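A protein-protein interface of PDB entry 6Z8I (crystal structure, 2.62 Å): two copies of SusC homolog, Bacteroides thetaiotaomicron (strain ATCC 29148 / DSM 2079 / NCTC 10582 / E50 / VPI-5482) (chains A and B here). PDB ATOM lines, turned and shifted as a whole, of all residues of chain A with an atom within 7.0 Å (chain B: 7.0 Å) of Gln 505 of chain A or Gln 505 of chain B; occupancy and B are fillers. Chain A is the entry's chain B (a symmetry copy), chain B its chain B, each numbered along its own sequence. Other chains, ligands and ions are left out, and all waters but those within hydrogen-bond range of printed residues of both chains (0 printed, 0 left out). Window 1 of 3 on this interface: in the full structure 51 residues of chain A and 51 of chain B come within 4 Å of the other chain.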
ATOM      1  N   THR A 448      20.375  -3.229 -30.286  1.00  0.00           N
ATOM      2  CA  THR A 448      19.133  -2.733 -29.710  1.00  0.00           C
ATOM      3  C   THR A 448      19.364  -1.281 -29.315  1.00  0.00           C
ATOM      4  O   THR A 448      20.180  -0.996 -28.427  1.00  0.00           O
ATOM      5  CB  THR A 448      18.707  -3.574 -28.494  1.00  0.00           C
ATOM      6  OG1 THR A 448      18.369  -4.910 -28.905  1.00  0.00           O
ATOM      7  CG2 THR A 448      17.507  -2.953 -27.782  1.00  0.00           C
ATOM      8  N   TYR A 476      18.800  11.522 -25.494  1.00  0.00           N
ATOM      9  CA  TYR A 476      19.608  10.440 -24.947  1.00  0.00           C
ATOM     10  C   TYR A 476      19.302   9.150 -25.697  1.00  0.00           C
ATOM     11  O   TYR A 476      18.150   8.704 -25.733  1.00  0.00           O
ATOM     12  CB  TYR A 476      19.357  10.245 -23.454  1.00  0.00           C
ATOM     13  CG  TYR A 476      19.977   8.969 -22.970  1.00  0.00           C
ATOM     14  CD1 TYR A 476      19.229   8.000 -22.317  1.00  0.00           C
ATOM     15  CD2 TYR A 476      21.316   8.714 -23.205  1.00  0.00           C
ATOM     16  CE1 TYR A 476      19.808   6.830 -21.897  1.00  0.00           C
ATOM     17  CE2 TYR A 476      21.898   7.556 -22.794  1.00  0.00           C
ATOM     18  CZ  TYR A 476      21.149   6.613 -22.137  1.00  0.00           C
ATOM     19  OH  TYR A 476      21.765   5.444 -21.736  1.00  0.00           O
ATOM     20  N   ALA A 477      20.335   8.561 -26.296  1.00  0.00           N
ATOM     21  CA  ALA A 477      20.240   7.299 -27.007  1.00  0.00           C
ATOM     22  C   ALA A 477      21.355   6.380 -26.543  1.00  0.00           C
ATOM     23  O   ALA A 477      22.420   6.840 -26.110  1.00  0.00           O
ATOM     24  CB  ALA A 477      20.344   7.475 -28.512  1.00  0.00           C
ATOM     25  N   ASN A 478      21.107   5.076 -26.647  1.00  0.00           N
ATOM     26  CA  ASN A 478      22.107   4.096 -26.265  1.00  0.00           C
ATOM     27  C   ASN A 478      21.943   2.864 -27.146  1.00  0.00           C
ATOM     28  O   ASN A 478      20.825   2.396 -27.392  1.00  0.00           O
ATOM     29  CB  ASN A 478      22.038   3.778 -24.758  1.00  0.00           C
ATOM     30  CG  ASN A 478      20.850   2.892 -24.361  1.00  0.00           C
ATOM     31  OD1 ASN A 478      20.544   1.869 -24.995  1.00  0.00           O
ATOM     32  ND2 ASN A 478      20.244   3.235 -23.257  1.00  0.00           N
ATOM     33  N   LYS A 479      23.068   2.366 -27.651  1.00  0.00           N
ATOM     34  CA  LYS A 479      23.074   1.211 -28.529  1.00  0.00           C
ATOM     35  C   LYS A 479      23.843   0.089 -27.843  1.00  0.00           C
ATOM     36  O   LYS A 479      24.857   0.328 -27.178  1.00  0.00           O
ATOM     37  CB  LYS A 479      23.689   1.551 -29.903  1.00  0.00           C
ATOM     38  CG  LYS A 479      23.404   0.519 -31.009  1.00  0.00           C
ATOM     39  CD  LYS A 479      23.700   1.038 -32.428  1.00  0.00           C
ATOM     40  CE  LYS A 479      25.026   0.489 -32.912  1.00  0.00           C
ATOM     41  NZ  LYS A 479      25.070   0.250 -34.380  1.00  0.00           N
ATOM     42  N   GLN A 480      23.335  -1.128 -27.997  1.00  0.00           N
ATOM     43  CA  GLN A 480      23.825  -2.302 -27.300  1.00  0.00           C
ATOM     44  C   GLN A 480      23.872  -3.423 -28.318  1.00  0.00           C
ATOM     45  O   GLN A 480      22.975  -3.521 -29.159  1.00  0.00           O
ATOM     46  CB  GLN A 480      22.891  -2.644 -26.124  1.00  0.00           C
ATOM     47  CG  GLN A 480      23.293  -3.836 -25.288  1.00  0.00           C
ATOM     48  CD  GLN A 480      22.401  -5.024 -25.545  1.00  0.00           C
ATOM     49  OE1 GLN A 480      21.260  -5.066 -25.078  1.00  0.00           O
ATOM     50  NE2 GLN A 480      22.911  -5.998 -26.309  1.00  0.00           N
ATOM     51  N   ALA A 481      24.923  -4.241 -28.283  1.00  0.00           N
ATOM     52  CA  ALA A 481      24.950  -5.388 -29.189  1.00  0.00           C
ATOM     53  C   ALA A 481      26.026  -6.395 -28.790  1.00  0.00           C
ATOM     54  O   ALA A 481      26.992  -6.074 -28.090  1.00  0.00           O
ATOM     55  CB  ALA A 481      25.177  -4.960 -30.640  1.00  0.00           C
ATOM     56  N   ALA A 503      30.805  -7.706 -26.797  1.00  0.00           N
ATOM     57  CA  ALA A 503      29.632  -7.067 -26.223  1.00  0.00           C
ATOM     58  C   ALA A 503      29.885  -5.561 -26.240  1.00  0.00           C
ATOM     59  O   ALA A 503      30.620  -5.049 -25.393  1.00  0.00           O
ATOM     60  CB  ALA A 503      29.384  -7.588 -24.809  1.00  0.00           C
ATOM     61  N   LYS A 504      29.273  -4.855 -27.205  1.00  0.00           N
ATOM     62  CA  LYS A 504      29.519  -3.432 -27.431  1.00  0.00           C
ATOM     63  C   LYS A 504      28.402  -2.594 -26.805  1.00  0.00           C
ATOM     64  O   LYS A 504      27.216  -2.942 -26.888  1.00  0.00           O
ATOM     65  CB  LYS A 504      29.640  -3.107 -28.937  1.00  0.00           C
ATOM     66  CG  LYS A 504      31.029  -3.346 -29.618  1.00  0.00           C
ATOM     67  CD  LYS A 504      31.382  -2.275 -30.724  1.00  0.00           C
ATOM     68  CE  LYS A 504      32.320  -2.795 -31.873  1.00  0.00           C
ATOM     69  NZ  LYS A 504      31.657  -2.920 -33.258  1.00  0.00           N
ATOM     70  N   GLN A 505      28.786  -1.475 -26.194  1.00  0.00           N
ATOM     71  CA  GLN A 505      27.847  -0.499 -25.657  1.00  0.00           C
ATOM     72  C   GLN A 505      28.217   0.911 -26.114  1.00  0.00           C
ATOM     73  O   GLN A 505      29.397   1.260 -26.176  1.00  0.00           O
ATOM     74  CB  GLN A 505      27.814  -0.545 -24.132  1.00  0.00           C
ATOM     75  CG  GLN A 505      26.925   0.543 -23.522  1.00  0.00           C
ATOM     76  CD  GLN A 505      25.446   0.345 -23.852  1.00  0.00           C
ATOM     77  OE1 GLN A 505      24.792   1.227 -24.391  1.00  0.00           O
ATOM     78  NE2 GLN A 505      24.928  -0.822 -23.536  1.00  0.00           N
ATOM     79  N   GLU A 506      27.199   1.721 -26.436  1.00  0.00           N
ATOM     80  CA  GLU A 506      27.361   3.129 -26.807  1.00  0.00           C
ATOM     81  C   GLU A 506      26.303   3.986 -26.127  1.00  0.00           C
ATOM     82  O   GLU A 506      25.147   3.570 -25.977  1.00  0.00           O
ATOM     83  CB  GLU A 506      27.277   3.338 -28.324  1.00  0.00           C
ATOM     84  CG  GLU A 506      28.051   2.304 -29.160  1.00  0.00           C
ATOM     85  CD  GLU A 506      28.086   2.635 -30.647  1.00  0.00           C
ATOM     86  OE1 GLU A 506      28.800   3.592 -31.049  1.00  0.00           O
ATOM     87  OE2 GLU A 506      27.370   1.938 -31.412  1.00  0.00           O
ATOM     88  N   HIS A 507      26.712   5.186 -25.722  1.00  0.00           N
ATOM     89  CA  HIS A 507      25.840   6.202 -25.144  1.00  0.00           C
ATOM     90  C   HIS A 507      26.084   7.550 -25.807  1.00  0.00           C
ATOM     91  O   HIS A 507      27.231   7.924 -26.055  1.00  0.00           O
ATOM     92  CB  HIS A 507      26.068   6.359 -23.639  1.00  0.00           C
ATOM     93  CG  HIS A 507      25.705   5.144 -22.845  1.00  0.00           C
ATOM     94  ND1 HIS A 507      24.466   4.985 -22.252  1.00  0.00           N
ATOM     95  CD2 HIS A 507      26.423   4.038 -22.532  1.00  0.00           C
ATOM     96  CE1 HIS A 507      24.435   3.825 -21.621  1.00  0.00           C
ATOM     97  NE2 HIS A 507      25.610   3.237 -21.769  1.00  0.00           N
ATOM     98  N   TRP A 508      24.992   8.267 -26.092  1.00  0.00           N
ATOM     99  CA  TRP A 508      25.011   9.649 -26.577  1.00  0.00           C
ATOM    100  C   TRP A 508      23.952  10.416 -25.801  1.00  0.00           C
ATOM    101  O   TRP A 508      22.758  10.178 -26.012  1.00  0.00           O
ATOM    102  CB  TRP A 508      24.677   9.745 -28.061  1.00  0.00           C
ATOM    103  CG  TRP A 508      25.393   8.870 -29.026  1.00  0.00           C
ATOM    104  CD1 TRP A 508      26.444   9.224 -29.791  1.00  0.00           C
ATOM    105  CD2 TRP A 508      25.053   7.530 -29.406  1.00  0.00           C
ATOM    106  NE1 TRP A 508      26.820   8.182 -30.598  1.00  0.00           N
ATOM    107  CE2 TRP A 508      25.980   7.127 -30.383  1.00  0.00           C
ATOM    108  CE3 TRP A 508      24.069   6.624 -28.998  1.00  0.00           C
ATOM    109  CZ2 TRP A 508      25.962   5.859 -30.963  1.00  0.00           C
ATOM    110  CZ3 TRP A 508      24.049   5.360 -29.577  1.00  0.00           C
ATOM    111  CH2 TRP A 508      24.995   4.994 -30.552  1.00  0.00           C
ATOM    112  N   SER A 542      30.206   8.308 -25.168  1.00  0.00           N
ATOM    113  CA  SER A 542      31.016   7.266 -24.551  1.00  0.00           C
ATOM    114  C   SER A 542      30.645   5.937 -25.184  1.00  0.00           C
ATOM    115  O   SER A 542      29.465   5.668 -25.426  1.00  0.00           O
ATOM    116  CB  SER A 542      30.794   7.176 -23.037  1.00  0.00           C
ATOM    117  OG  SER A 542      29.439   6.878 -22.755  1.00  0.00           O
ATOM    118  N   HIS A 543      31.653   5.109 -25.445  1.00  0.00           N
ATOM    119  CA  HIS A 543      31.414   3.731 -25.832  1.00  0.00           C
ATOM    120  C   HIS A 543      32.449   2.868 -25.120  1.00  0.00           C
ATOM    121  O   HIS A 543      33.399   3.380 -24.517  1.00  0.00           O
ATOM    122  CB  HIS A 543      31.432   3.566 -27.360  1.00  0.00           C
ATOM    123  CG  HIS A 543      32.762   3.826 -27.981  1.00  0.00           C
ATOM    124  ND1 HIS A 543      33.614   4.812 -27.530  1.00  0.00           N
ATOM    125  CD2 HIS A 543      33.396   3.219 -29.012  1.00  0.00           C
ATOM    126  CE1 HIS A 543      34.720   4.794 -28.254  1.00  0.00           C
ATOM    127  NE2 HIS A 543      34.612   3.836 -29.159  1.00  0.00           N
ATOM    128  N   PHE A 544      32.225   1.547 -25.142  1.00  0.00           N
ATOM    129  CA  PHE A 544      33.116   0.571 -24.515  1.00  0.00           C
ATOM    130  C   PHE A 544      32.604  -0.832 -24.787  1.00  0.00           C
ATOM    131  O   PHE A 544      31.398  -1.020 -24.991  1.00  0.00           O
ATOM    132  CB  PHE A 544      33.254   0.800 -23.003  1.00  0.00           C
ATOM    133  CG  PHE A 544      31.954   0.700 -22.235  1.00  0.00           C
ATOM    134  CD1 PHE A 544      31.522  -0.520 -21.732  1.00  0.00           C
ATOM    135  CD2 PHE A 544      31.173   1.831 -21.999  1.00  0.00           C
ATOM    136  CE1 PHE A 544      30.328  -0.614 -21.010  1.00  0.00           C
ATOM    137  CE2 PHE A 544      29.962   1.749 -21.292  1.00  0.00           C
ATOM    138  CZ  PHE A 544      29.550   0.528 -20.797  1.00  0.00           C
ATOM    139  N   SER A 545      33.507  -1.818 -24.796  1.00  0.00           N
ATOM    140  CA  SER A 545      33.109  -3.194 -25.079  1.00  0.00           C
ATOM    141  C   SER A 545      33.968  -4.185 -24.302  1.00  0.00           C
ATOM    142  O   SER A 545      34.975  -3.834 -23.678  1.00  0.00           O
ATOM    143  CB  SER A 545      33.186  -3.503 -26.582  1.00  0.00           C
ATOM    144  OG  SER A 545      34.434  -3.126 -27.155  1.00  0.00           O
ATOM    145  N   GLY A 546      33.532  -5.439 -24.350  1.00  0.00           N
ATOM    146  CA  GLY A 546      34.292  -6.570 -23.873  1.00  0.00           C
ATOM    147  C   GLY A 546      34.347  -7.659 -24.926  1.00  0.00           C
ATOM    148  O   GLY A 546      33.323  -8.077 -25.491  1.00  0.00           O
ATOM    149  N   THR B 448      25.399   6.058 -13.866  1.00  0.00           N
ATOM    150  CA  THR B 448      24.361   6.872 -14.486  1.00  0.00           C
ATOM    151  C   THR B 448      23.235   5.934 -14.898  1.00  0.00           C
ATOM    152  O   THR B 448      23.425   5.071 -15.767  1.00  0.00           O
ATOM    153  CB  THR B 448      24.908   7.643 -15.700  1.00  0.00           C
ATOM    154  OG1 THR B 448      25.880   8.615 -15.277  1.00  0.00           O
ATOM    155  CG2 THR B 448      23.788   8.355 -16.455  1.00  0.00           C
ATOM    156  N   TYR B 476      12.003  -0.093 -18.943  1.00  0.00           N
ATOM    157  CA  TYR B 476      13.360  -0.254 -19.449  1.00  0.00           C
ATOM    158  C   TYR B 476      14.298   0.673 -18.687  1.00  0.00           C
ATOM    159  O   TYR B 476      14.103   1.893 -18.676  1.00  0.00           O
ATOM    160  CB  TYR B 476      13.444   0.037 -20.945  1.00  0.00           C
ATOM    161  CG  TYR B 476      14.873   0.136 -21.390  1.00  0.00           C
ATOM    162  CD1 TYR B 476      15.352   1.259 -22.048  1.00  0.00           C
ATOM    163  CD2 TYR B 476      15.760  -0.888 -21.113  1.00  0.00           C
ATOM    164  CE1 TYR B 476      16.665   1.342 -22.433  1.00  0.00           C
ATOM    165  CE2 TYR B 476      17.065  -0.814 -21.487  1.00  0.00           C
ATOM    166  CZ  TYR B 476      17.521   0.297 -22.150  1.00  0.00           C
ATOM    167  OH  TYR B 476      18.852   0.347 -22.514  1.00  0.00           O
ATOM    168  N   ALA B 477      15.310   0.087 -18.049  1.00  0.00           N
ATOM    169  CA  ALA B 477      16.332   0.817 -17.321  1.00  0.00           C
ATOM    170  C   ALA B 477      17.700   0.309 -17.737  1.00  0.00           C
ATOM    171  O   ALA B 477      17.851  -0.850 -18.147  1.00  0.00           O
ATOM    172  CB  ALA B 477      16.189   0.663 -15.816  1.00  0.00           C
ATOM    173  N   ASN B 478      18.699   1.182 -17.619  1.00  0.00           N
ATOM    174  CA  ASN B 478      20.059   0.806 -17.956  1.00  0.00           C
ATOM    175  C   ASN B 478      21.015   1.583 -17.060  1.00  0.00           C
ATOM    176  O   ASN B 478      20.850   2.788 -16.838  1.00  0.00           O
ATOM    177  CB  ASN B 478      20.341   1.001 -19.459  1.00  0.00           C
ATOM    178  CG  ASN B 478      20.520   2.467 -19.875  1.00  0.00           C
ATOM    179  OD1 ASN B 478      21.232   3.257 -19.233  1.00  0.00           O
ATOM    180  ND2 ASN B 478      19.951   2.799 -21.002  1.00  0.00           N
ATOM    181  N   LYS B 479      21.997   0.870 -16.515  1.00  0.00           N
ATOM    182  CA  LYS B 479      22.973   1.462 -15.618  1.00  0.00           C
ATOM    183  C   LYS B 479      24.348   1.351 -16.263  1.00  0.00           C
ATOM    184  O   LYS B 479      24.671   0.345 -16.903  1.00  0.00           O
ATOM    185  CB  LYS B 479      22.949   0.782 -14.233  1.00  0.00           C
ATOM    186  CG  LYS B 479      23.665   1.565 -13.119  1.00  0.00           C
ATOM    187  CD  LYS B 479      23.326   1.072 -11.701  1.00  0.00           C
ATOM    188  CE  LYS B 479      24.453   0.211 -11.170  1.00  0.00           C
ATOM    189  NZ  LYS B 479      24.640   0.318  -9.698  1.00  0.00           N
ATOM    190  N   GLN B 480      25.139   2.405 -16.104  1.00  0.00           N
ATOM    191  CA  GLN B 480      26.419   2.562 -16.767  1.00  0.00           C
ATOM    192  C   GLN B 480      27.383   3.103 -15.730  1.00  0.00           C
ATOM    193  O   GLN B 480      26.991   3.941 -14.914  1.00  0.00           O
ATOM    194  CB  GLN B 480      26.278   3.522 -17.964  1.00  0.00           C
ATOM    195  CG  GLN B 480      27.534   3.762 -18.769  1.00  0.00           C
ATOM    196  CD  GLN B 480      28.103   5.135 -18.517  1.00  0.00           C
ATOM    197  OE1 GLN B 480      27.579   6.133 -19.016  1.00  0.00           O
ATOM    198  NE2 GLN B 480      29.180   5.198 -17.724  1.00  0.00           N
ATOM    199  N   ALA B 481      28.619   2.607 -15.722  1.00  0.00           N
ATOM    200  CA  ALA B 481      29.597   3.176 -14.797  1.00  0.00           C
ATOM    201  C   ALA B 481      31.019   2.748 -15.148  1.00  0.00           C
ATOM    202  O   ALA B 481      31.249   1.741 -15.826  1.00  0.00           O
ATOM    203  CB  ALA B 481      29.300   2.789 -13.347  1.00  0.00           C
ATOM    204  N   ALA B 503      34.614  -0.752 -16.982  1.00  0.00           N
ATOM    205  CA  ALA B 503      33.488  -0.070 -17.600  1.00  0.00           C
ATOM    206  C   ALA B 503      32.315  -1.046 -17.600  1.00  0.00           C
ATOM    207  O   ALA B 503      32.266  -1.954 -18.434  1.00  0.00           O
ATOM    208  CB  ALA B 503      33.854   0.384 -19.012  1.00  0.00           C
ATOM    209  N   LYS B 504      31.369  -0.858 -16.665  1.00  0.00           N
ATOM    210  CA  LYS B 504      30.258  -1.784 -16.456  1.00  0.00           C
ATOM    211  C   LYS B 504      28.989  -1.252 -17.127  1.00  0.00           C
ATOM    212  O   LYS B 504      28.691  -0.050 -17.072  1.00  0.00           O
ATOM    213  CB  LYS B 504      29.995  -2.027 -14.953  1.00  0.00           C
ATOM    214  CG  LYS B 504      30.881  -3.095 -14.228  1.00  0.00           C
ATOM    215  CD  LYS B 504      30.102  -3.922 -13.130  1.00  0.00           C
ATOM    216  CE  LYS B 504      30.990  -4.450 -11.947  1.00  0.00           C
ATOM    217  NZ  LYS B 504      30.725  -3.792 -10.579  1.00  0.00           N
ATOM    218  N   GLN B 505      28.234  -2.157 -17.745  1.00  0.00           N
ATOM    219  CA  GLN B 505      26.933  -1.846 -18.324  1.00  0.00           C
ATOM    220  C   GLN B 505      25.889  -2.869 -17.881  1.00  0.00           C
ATOM    221  O   GLN B 505      26.180  -4.062 -17.790  1.00  0.00           O
ATOM    222  CB  GLN B 505      27.000  -1.820 -19.849  1.00  0.00           C
ATOM    223  CG  GLN B 505      25.631  -1.610 -20.502  1.00  0.00           C
ATOM    224  CD  GLN B 505      25.048  -0.228 -20.211  1.00  0.00           C
ATOM    225  OE1 GLN B 505      23.942  -0.098 -19.706  1.00  0.00           O
ATOM    226  NE2 GLN B 505      25.804   0.803 -20.522  1.00  0.00           N
ATOM    227  N   GLU B 506      24.668  -2.393 -17.601  1.00  0.00           N
ATOM    228  CA  GLU B 506      23.523  -3.236 -17.249  1.00  0.00           C
ATOM    229  C   GLU B 506      22.270  -2.765 -17.972  1.00  0.00           C
ATOM    230  O   GLU B 506      22.051  -1.559 -18.149  1.00  0.00           O
ATOM    231  CB  GLU B 506      23.257  -3.244 -15.738  1.00  0.00           C
ATOM    232  CG  GLU B 506      24.515  -3.377 -14.864  1.00  0.00           C
ATOM    233  CD  GLU B 506      24.205  -3.550 -13.382  1.00  0.00           C
ATOM    234  OE1 GLU B 506      23.726  -4.642 -12.976  1.00  0.00           O
ATOM    235  OE2 GLU B 506      24.425  -2.568 -12.626  1.00  0.00           O
ATOM    236  N   HIS B 507      21.451  -3.730 -18.385  1.00  0.00           N
ATOM    237  CA  HIS B 507      20.151  -3.497 -19.004  1.00  0.00           C
ATOM    238  C   HIS B 507      19.091  -4.376 -18.357  1.00  0.00           C
ATOM    239  O   HIS B 507      19.338  -5.551 -18.082  1.00  0.00           O
ATOM    240  CB  HIS B 507      20.173  -3.798 -20.505  1.00  0.00           C
ATOM    241  CG  HIS B 507      21.063  -2.886 -21.289  1.00  0.00           C
ATOM    242  ND1 HIS B 507      20.593  -1.746 -21.914  1.00  0.00           N
ATOM    243  CD2 HIS B 507      22.388  -2.954 -21.563  1.00  0.00           C
ATOM    244  CE1 HIS B 507      21.597  -1.145 -22.526  1.00  0.00           C
ATOM    245  NE2 HIS B 507      22.692  -1.860 -22.335  1.00  0.00           N
ATOM    246  N   TRP B 508      17.914  -3.791 -18.115  1.00  0.00           N
ATOM    247  CA  TRP B 508      16.716  -4.495 -17.652  1.00  0.00           C
ATOM    248  C   TRP B 508      15.542  -3.979 -18.471  1.00  0.00           C
ATOM    249  O   TRP B 508      15.141  -2.825 -18.290  1.00  0.00           O
ATOM    250  CB  TRP B 508      16.423  -4.230 -16.181  1.00  0.00           C
ATOM    251  CG  TRP B 508      17.511  -4.392 -15.181  1.00  0.00           C
ATOM    252  CD1 TRP B 508      17.712  -5.465 -14.392  1.00  0.00           C
ATOM    253  CD2 TRP B 508      18.486  -3.417 -14.789  1.00  0.00           C
ATOM    254  NE1 TRP B 508      18.778  -5.252 -13.558  1.00  0.00           N
ATOM    255  CE2 TRP B 508      19.273  -3.998 -13.780  1.00  0.00           C
ATOM    256  CE3 TRP B 508      18.785  -2.118 -15.210  1.00  0.00           C
ATOM    257  CZ2 TRP B 508      20.342  -3.335 -13.179  1.00  0.00           C
ATOM    258  CZ3 TRP B 508      19.851  -1.454 -14.611  1.00  0.00           C
ATOM    259  CH2 TRP B 508      20.615  -2.070 -13.604  1.00  0.00           C
ATOM    260  N   SER B 542      20.529  -8.330 -18.890  1.00  0.00           N
ATOM    261  CA  SER B 542      21.854  -8.514 -19.467  1.00  0.00           C
ATOM    262  C   SER B 542      22.797  -7.513 -18.823  1.00  0.00           C
ATOM    263  O   SER B 542      22.429  -6.354 -18.610  1.00  0.00           O
ATOM    264  CB  SER B 542      21.864  -8.301 -20.985  1.00  0.00           C
ATOM    265  OG  SER B 542      21.447  -6.986 -21.300  1.00  0.00           O
ATOM    266  N   HIS B 543      24.012  -7.962 -18.519  1.00  0.00           N
ATOM    267  CA  HIS B 543      25.071  -7.055 -18.117  1.00  0.00           C
ATOM    268  C   HIS B 543      26.357  -7.526 -18.785  1.00  0.00           C
ATOM    269  O   HIS B 543      26.410  -8.614 -19.369  1.00  0.00           O
ATOM    270  CB  HIS B 543      25.179  -6.963 -16.587  1.00  0.00           C
ATOM    271  CG  HIS B 543      25.606  -8.232 -15.933  1.00  0.00           C
ATOM    272  ND1 HIS B 543      25.196  -9.473 -16.375  1.00  0.00           N
ATOM    273  CD2 HIS B 543      26.420  -8.457 -14.873  1.00  0.00           C
ATOM    274  CE1 HIS B 543      25.747 -10.407 -15.620  1.00  0.00           C
ATOM    275  NE2 HIS B 543      26.495  -9.816 -14.703  1.00  0.00           N
ATOM    276  N   PHE B 544      27.385  -6.667 -18.748  1.00  0.00           N
ATOM    277  CA  PHE B 544      28.694  -6.954 -19.332  1.00  0.00           C
ATOM    278  C   PHE B 544      29.641  -5.801 -19.053  1.00  0.00           C
ATOM    279  O   PHE B 544      29.190  -4.661 -18.880  1.00  0.00           O
ATOM    280  CB  PHE B 544      28.609  -7.214 -20.844  1.00  0.00           C
ATOM    281  CG  PHE B 544      28.063  -6.054 -21.647  1.00  0.00           C
ATOM    282  CD1 PHE B 544      28.914  -5.074 -22.142  1.00  0.00           C
ATOM    283  CD2 PHE B 544      26.699  -5.953 -21.923  1.00  0.00           C
ATOM    284  CE1 PHE B 544      28.414  -4.007 -22.896  1.00  0.00           C
ATOM    285  CE2 PHE B 544      26.181  -4.877 -22.664  1.00  0.00           C
ATOM    286  CZ  PHE B 544      27.043  -3.914 -23.150  1.00  0.00           C
ATOM    287  N   SER B 545      30.946  -6.084 -19.002  1.00  0.00           N
ATOM    288  CA  SER B 545      31.926  -5.043 -18.707  1.00  0.00           C
ATOM    289  C   SER B 545      33.236  -5.298 -19.444  1.00  0.00           C
ATOM    290  O   SER B 545      33.458  -6.355 -20.044  1.00  0.00           O
ATOM    291  CB  SER B 545      32.189  -4.928 -17.198  1.00  0.00           C
ATOM    292  OG  SER B 545      32.475  -6.187 -16.596  1.00  0.00           O
ATOM    293  N   GLY B 546      34.098  -4.289 -19.387  1.00  0.00           N
ATOM    294  CA  GLY B 546      35.471  -4.383 -19.824  1.00  0.00           C
ATOM    295  C   GLY B 546      36.410  -3.865 -18.751  1.00  0.00           C
ATOM    296  O   GLY B 546      36.239  -2.761 -18.210  1.00  0.00           O
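The side-chain hydroxyl (OH) of Tyr 476 of chain B lies within hydrogen-bond range of the side-chain amide nitrogen (ND2) of Asn 478 of chain A (3.3 Å).
The side-chain hydroxyl of Tyr 476 of chain A lies within hydrogen-bond range of the side-chain amide nitrogen of Asn 478 of chain B (3.3 Å).
The side-chain amide nitrogen of Gln 505 of chain B lies within hydrogen-bond range of a ring nitrogen (NE2) of His 507 of chain A (2.7 Å).
The side-chain amide nitrogen of Gln 505 of chain A sits at hydrogen-bond distance from a ring nitrogen (NE2) of His 507 of chain B.
ND2 of Asn 478 of chain A sits close to ND2 of Asn 478 of chain B (2.3 Å).
The side-chain amide oxygen (OE1) of Gln 505 of chain B lies close to the backbone carbonyl oxygen (O) of Lys 479 of chain B, at 2.9 Å.
N of Ala 503 of chain B sits at hydrogen-bond distance from O of Gly 546 of chain B (2.9 Å).
The backbone NH (N) of His 507 of chain B sits at hydrogen-bond distance from the backbone carbonyl oxygen (O) of Ser 542 of chain B (2.8 Å).
ND2 of Asn 478 of chain A sits at hydrogen-bond distance from OH of Tyr 476 of chain A, 3.1 Å away.
O of Ala 481 of chain A lies within hydrogen-bond range of N of Lys 504 of chain A, 2.7 Å away.
The backbone carbonyl oxygen (O) of Gly 546 of chain A lies within hydrogen-bond range of the backbone NH (N) of Ala 503 of chain A (2.9 Å).
Gln 480 of chain A touches His 507 of chain B (CG to NE2, 3.6 Å).
Phe 544 of chain B touches Ala 503 of chain A (CE1 to O, 3.5 Å).
CZ of Phe 544 of chain B touches O of Lys 504 of chain A, at 3.9 Å.
Gln 505 of chain B touches Gln 505 of chain A.
Gln 505 of chain A touches Phe 544 of chain B (CB to CZ, 3.6 Å).
Gln 480 of chain B touches His 507 of chain A.
Ala 503 of chain B touches Phe 544 of chain A.
O of Lys 504 of chain B touches CZ of Phe 544 of chain A (3.9 Å).
Phe 544 of chain A touches Gln 505 of chain B (CZ to CB, 3.6 Å).
O of Ser 545 of chain A touches CA of Gly 546 of chain B, 3.9 Å away.
Of the printed residues of chain B, Lys 504 of chain A touches Phe 544.
Gln 505 of chain A touches just these residues of chain B: Gln 505, His 507 and Phe 544.
Of the printed residues of chain B, Ser 545 of chain A touches Gly 546 (3.9 Å).
Lys 479 of chain B touches none of the printed residues of chain A.
Gln 505 of chain B touches three residues of chain A.
Ser 542 of chain B touches none of the printed residues of chain A.
The nearest residue of chain A that does not touch Gln 505 of chain B is Gln 480 of chain A (5.8 Å).
Of the 18 printed residues of chain B, 10 touch a printed residue of chain A.
Hydrophobic or aromatic side chains of chain B within 4 Å of the printed part of chain A: Tyr 476, Ala 503, His 507 and Phe 544.
Of the 18 printed residues of chain A, 10 touch a printed residue of chain B.
Hydrophobic or aromatic side chains of chain A that line the printed part of chain B: Tyr 476, Ala 503, His 507 and Phe 544.
Among the printed residues, 16 pairs touch across the chains.
Gln 480 of chain A touches His 507 of chain B, and with the chains exchanged His 507 of chain A touches Gln 480 of chain B.
Ala 503 of chain A touches Phe 544 of chain B, and with the chains exchanged Phe 544 of chain A touches Ala 503 of chain B.
Gln 505 of chain B touches its own counterpart, Gln 505 of chain A.
Gln 505 of chain A touches His 507 of chain B, and with the chains exchanged His 507 of chain A touches Gln 505 of chain B.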
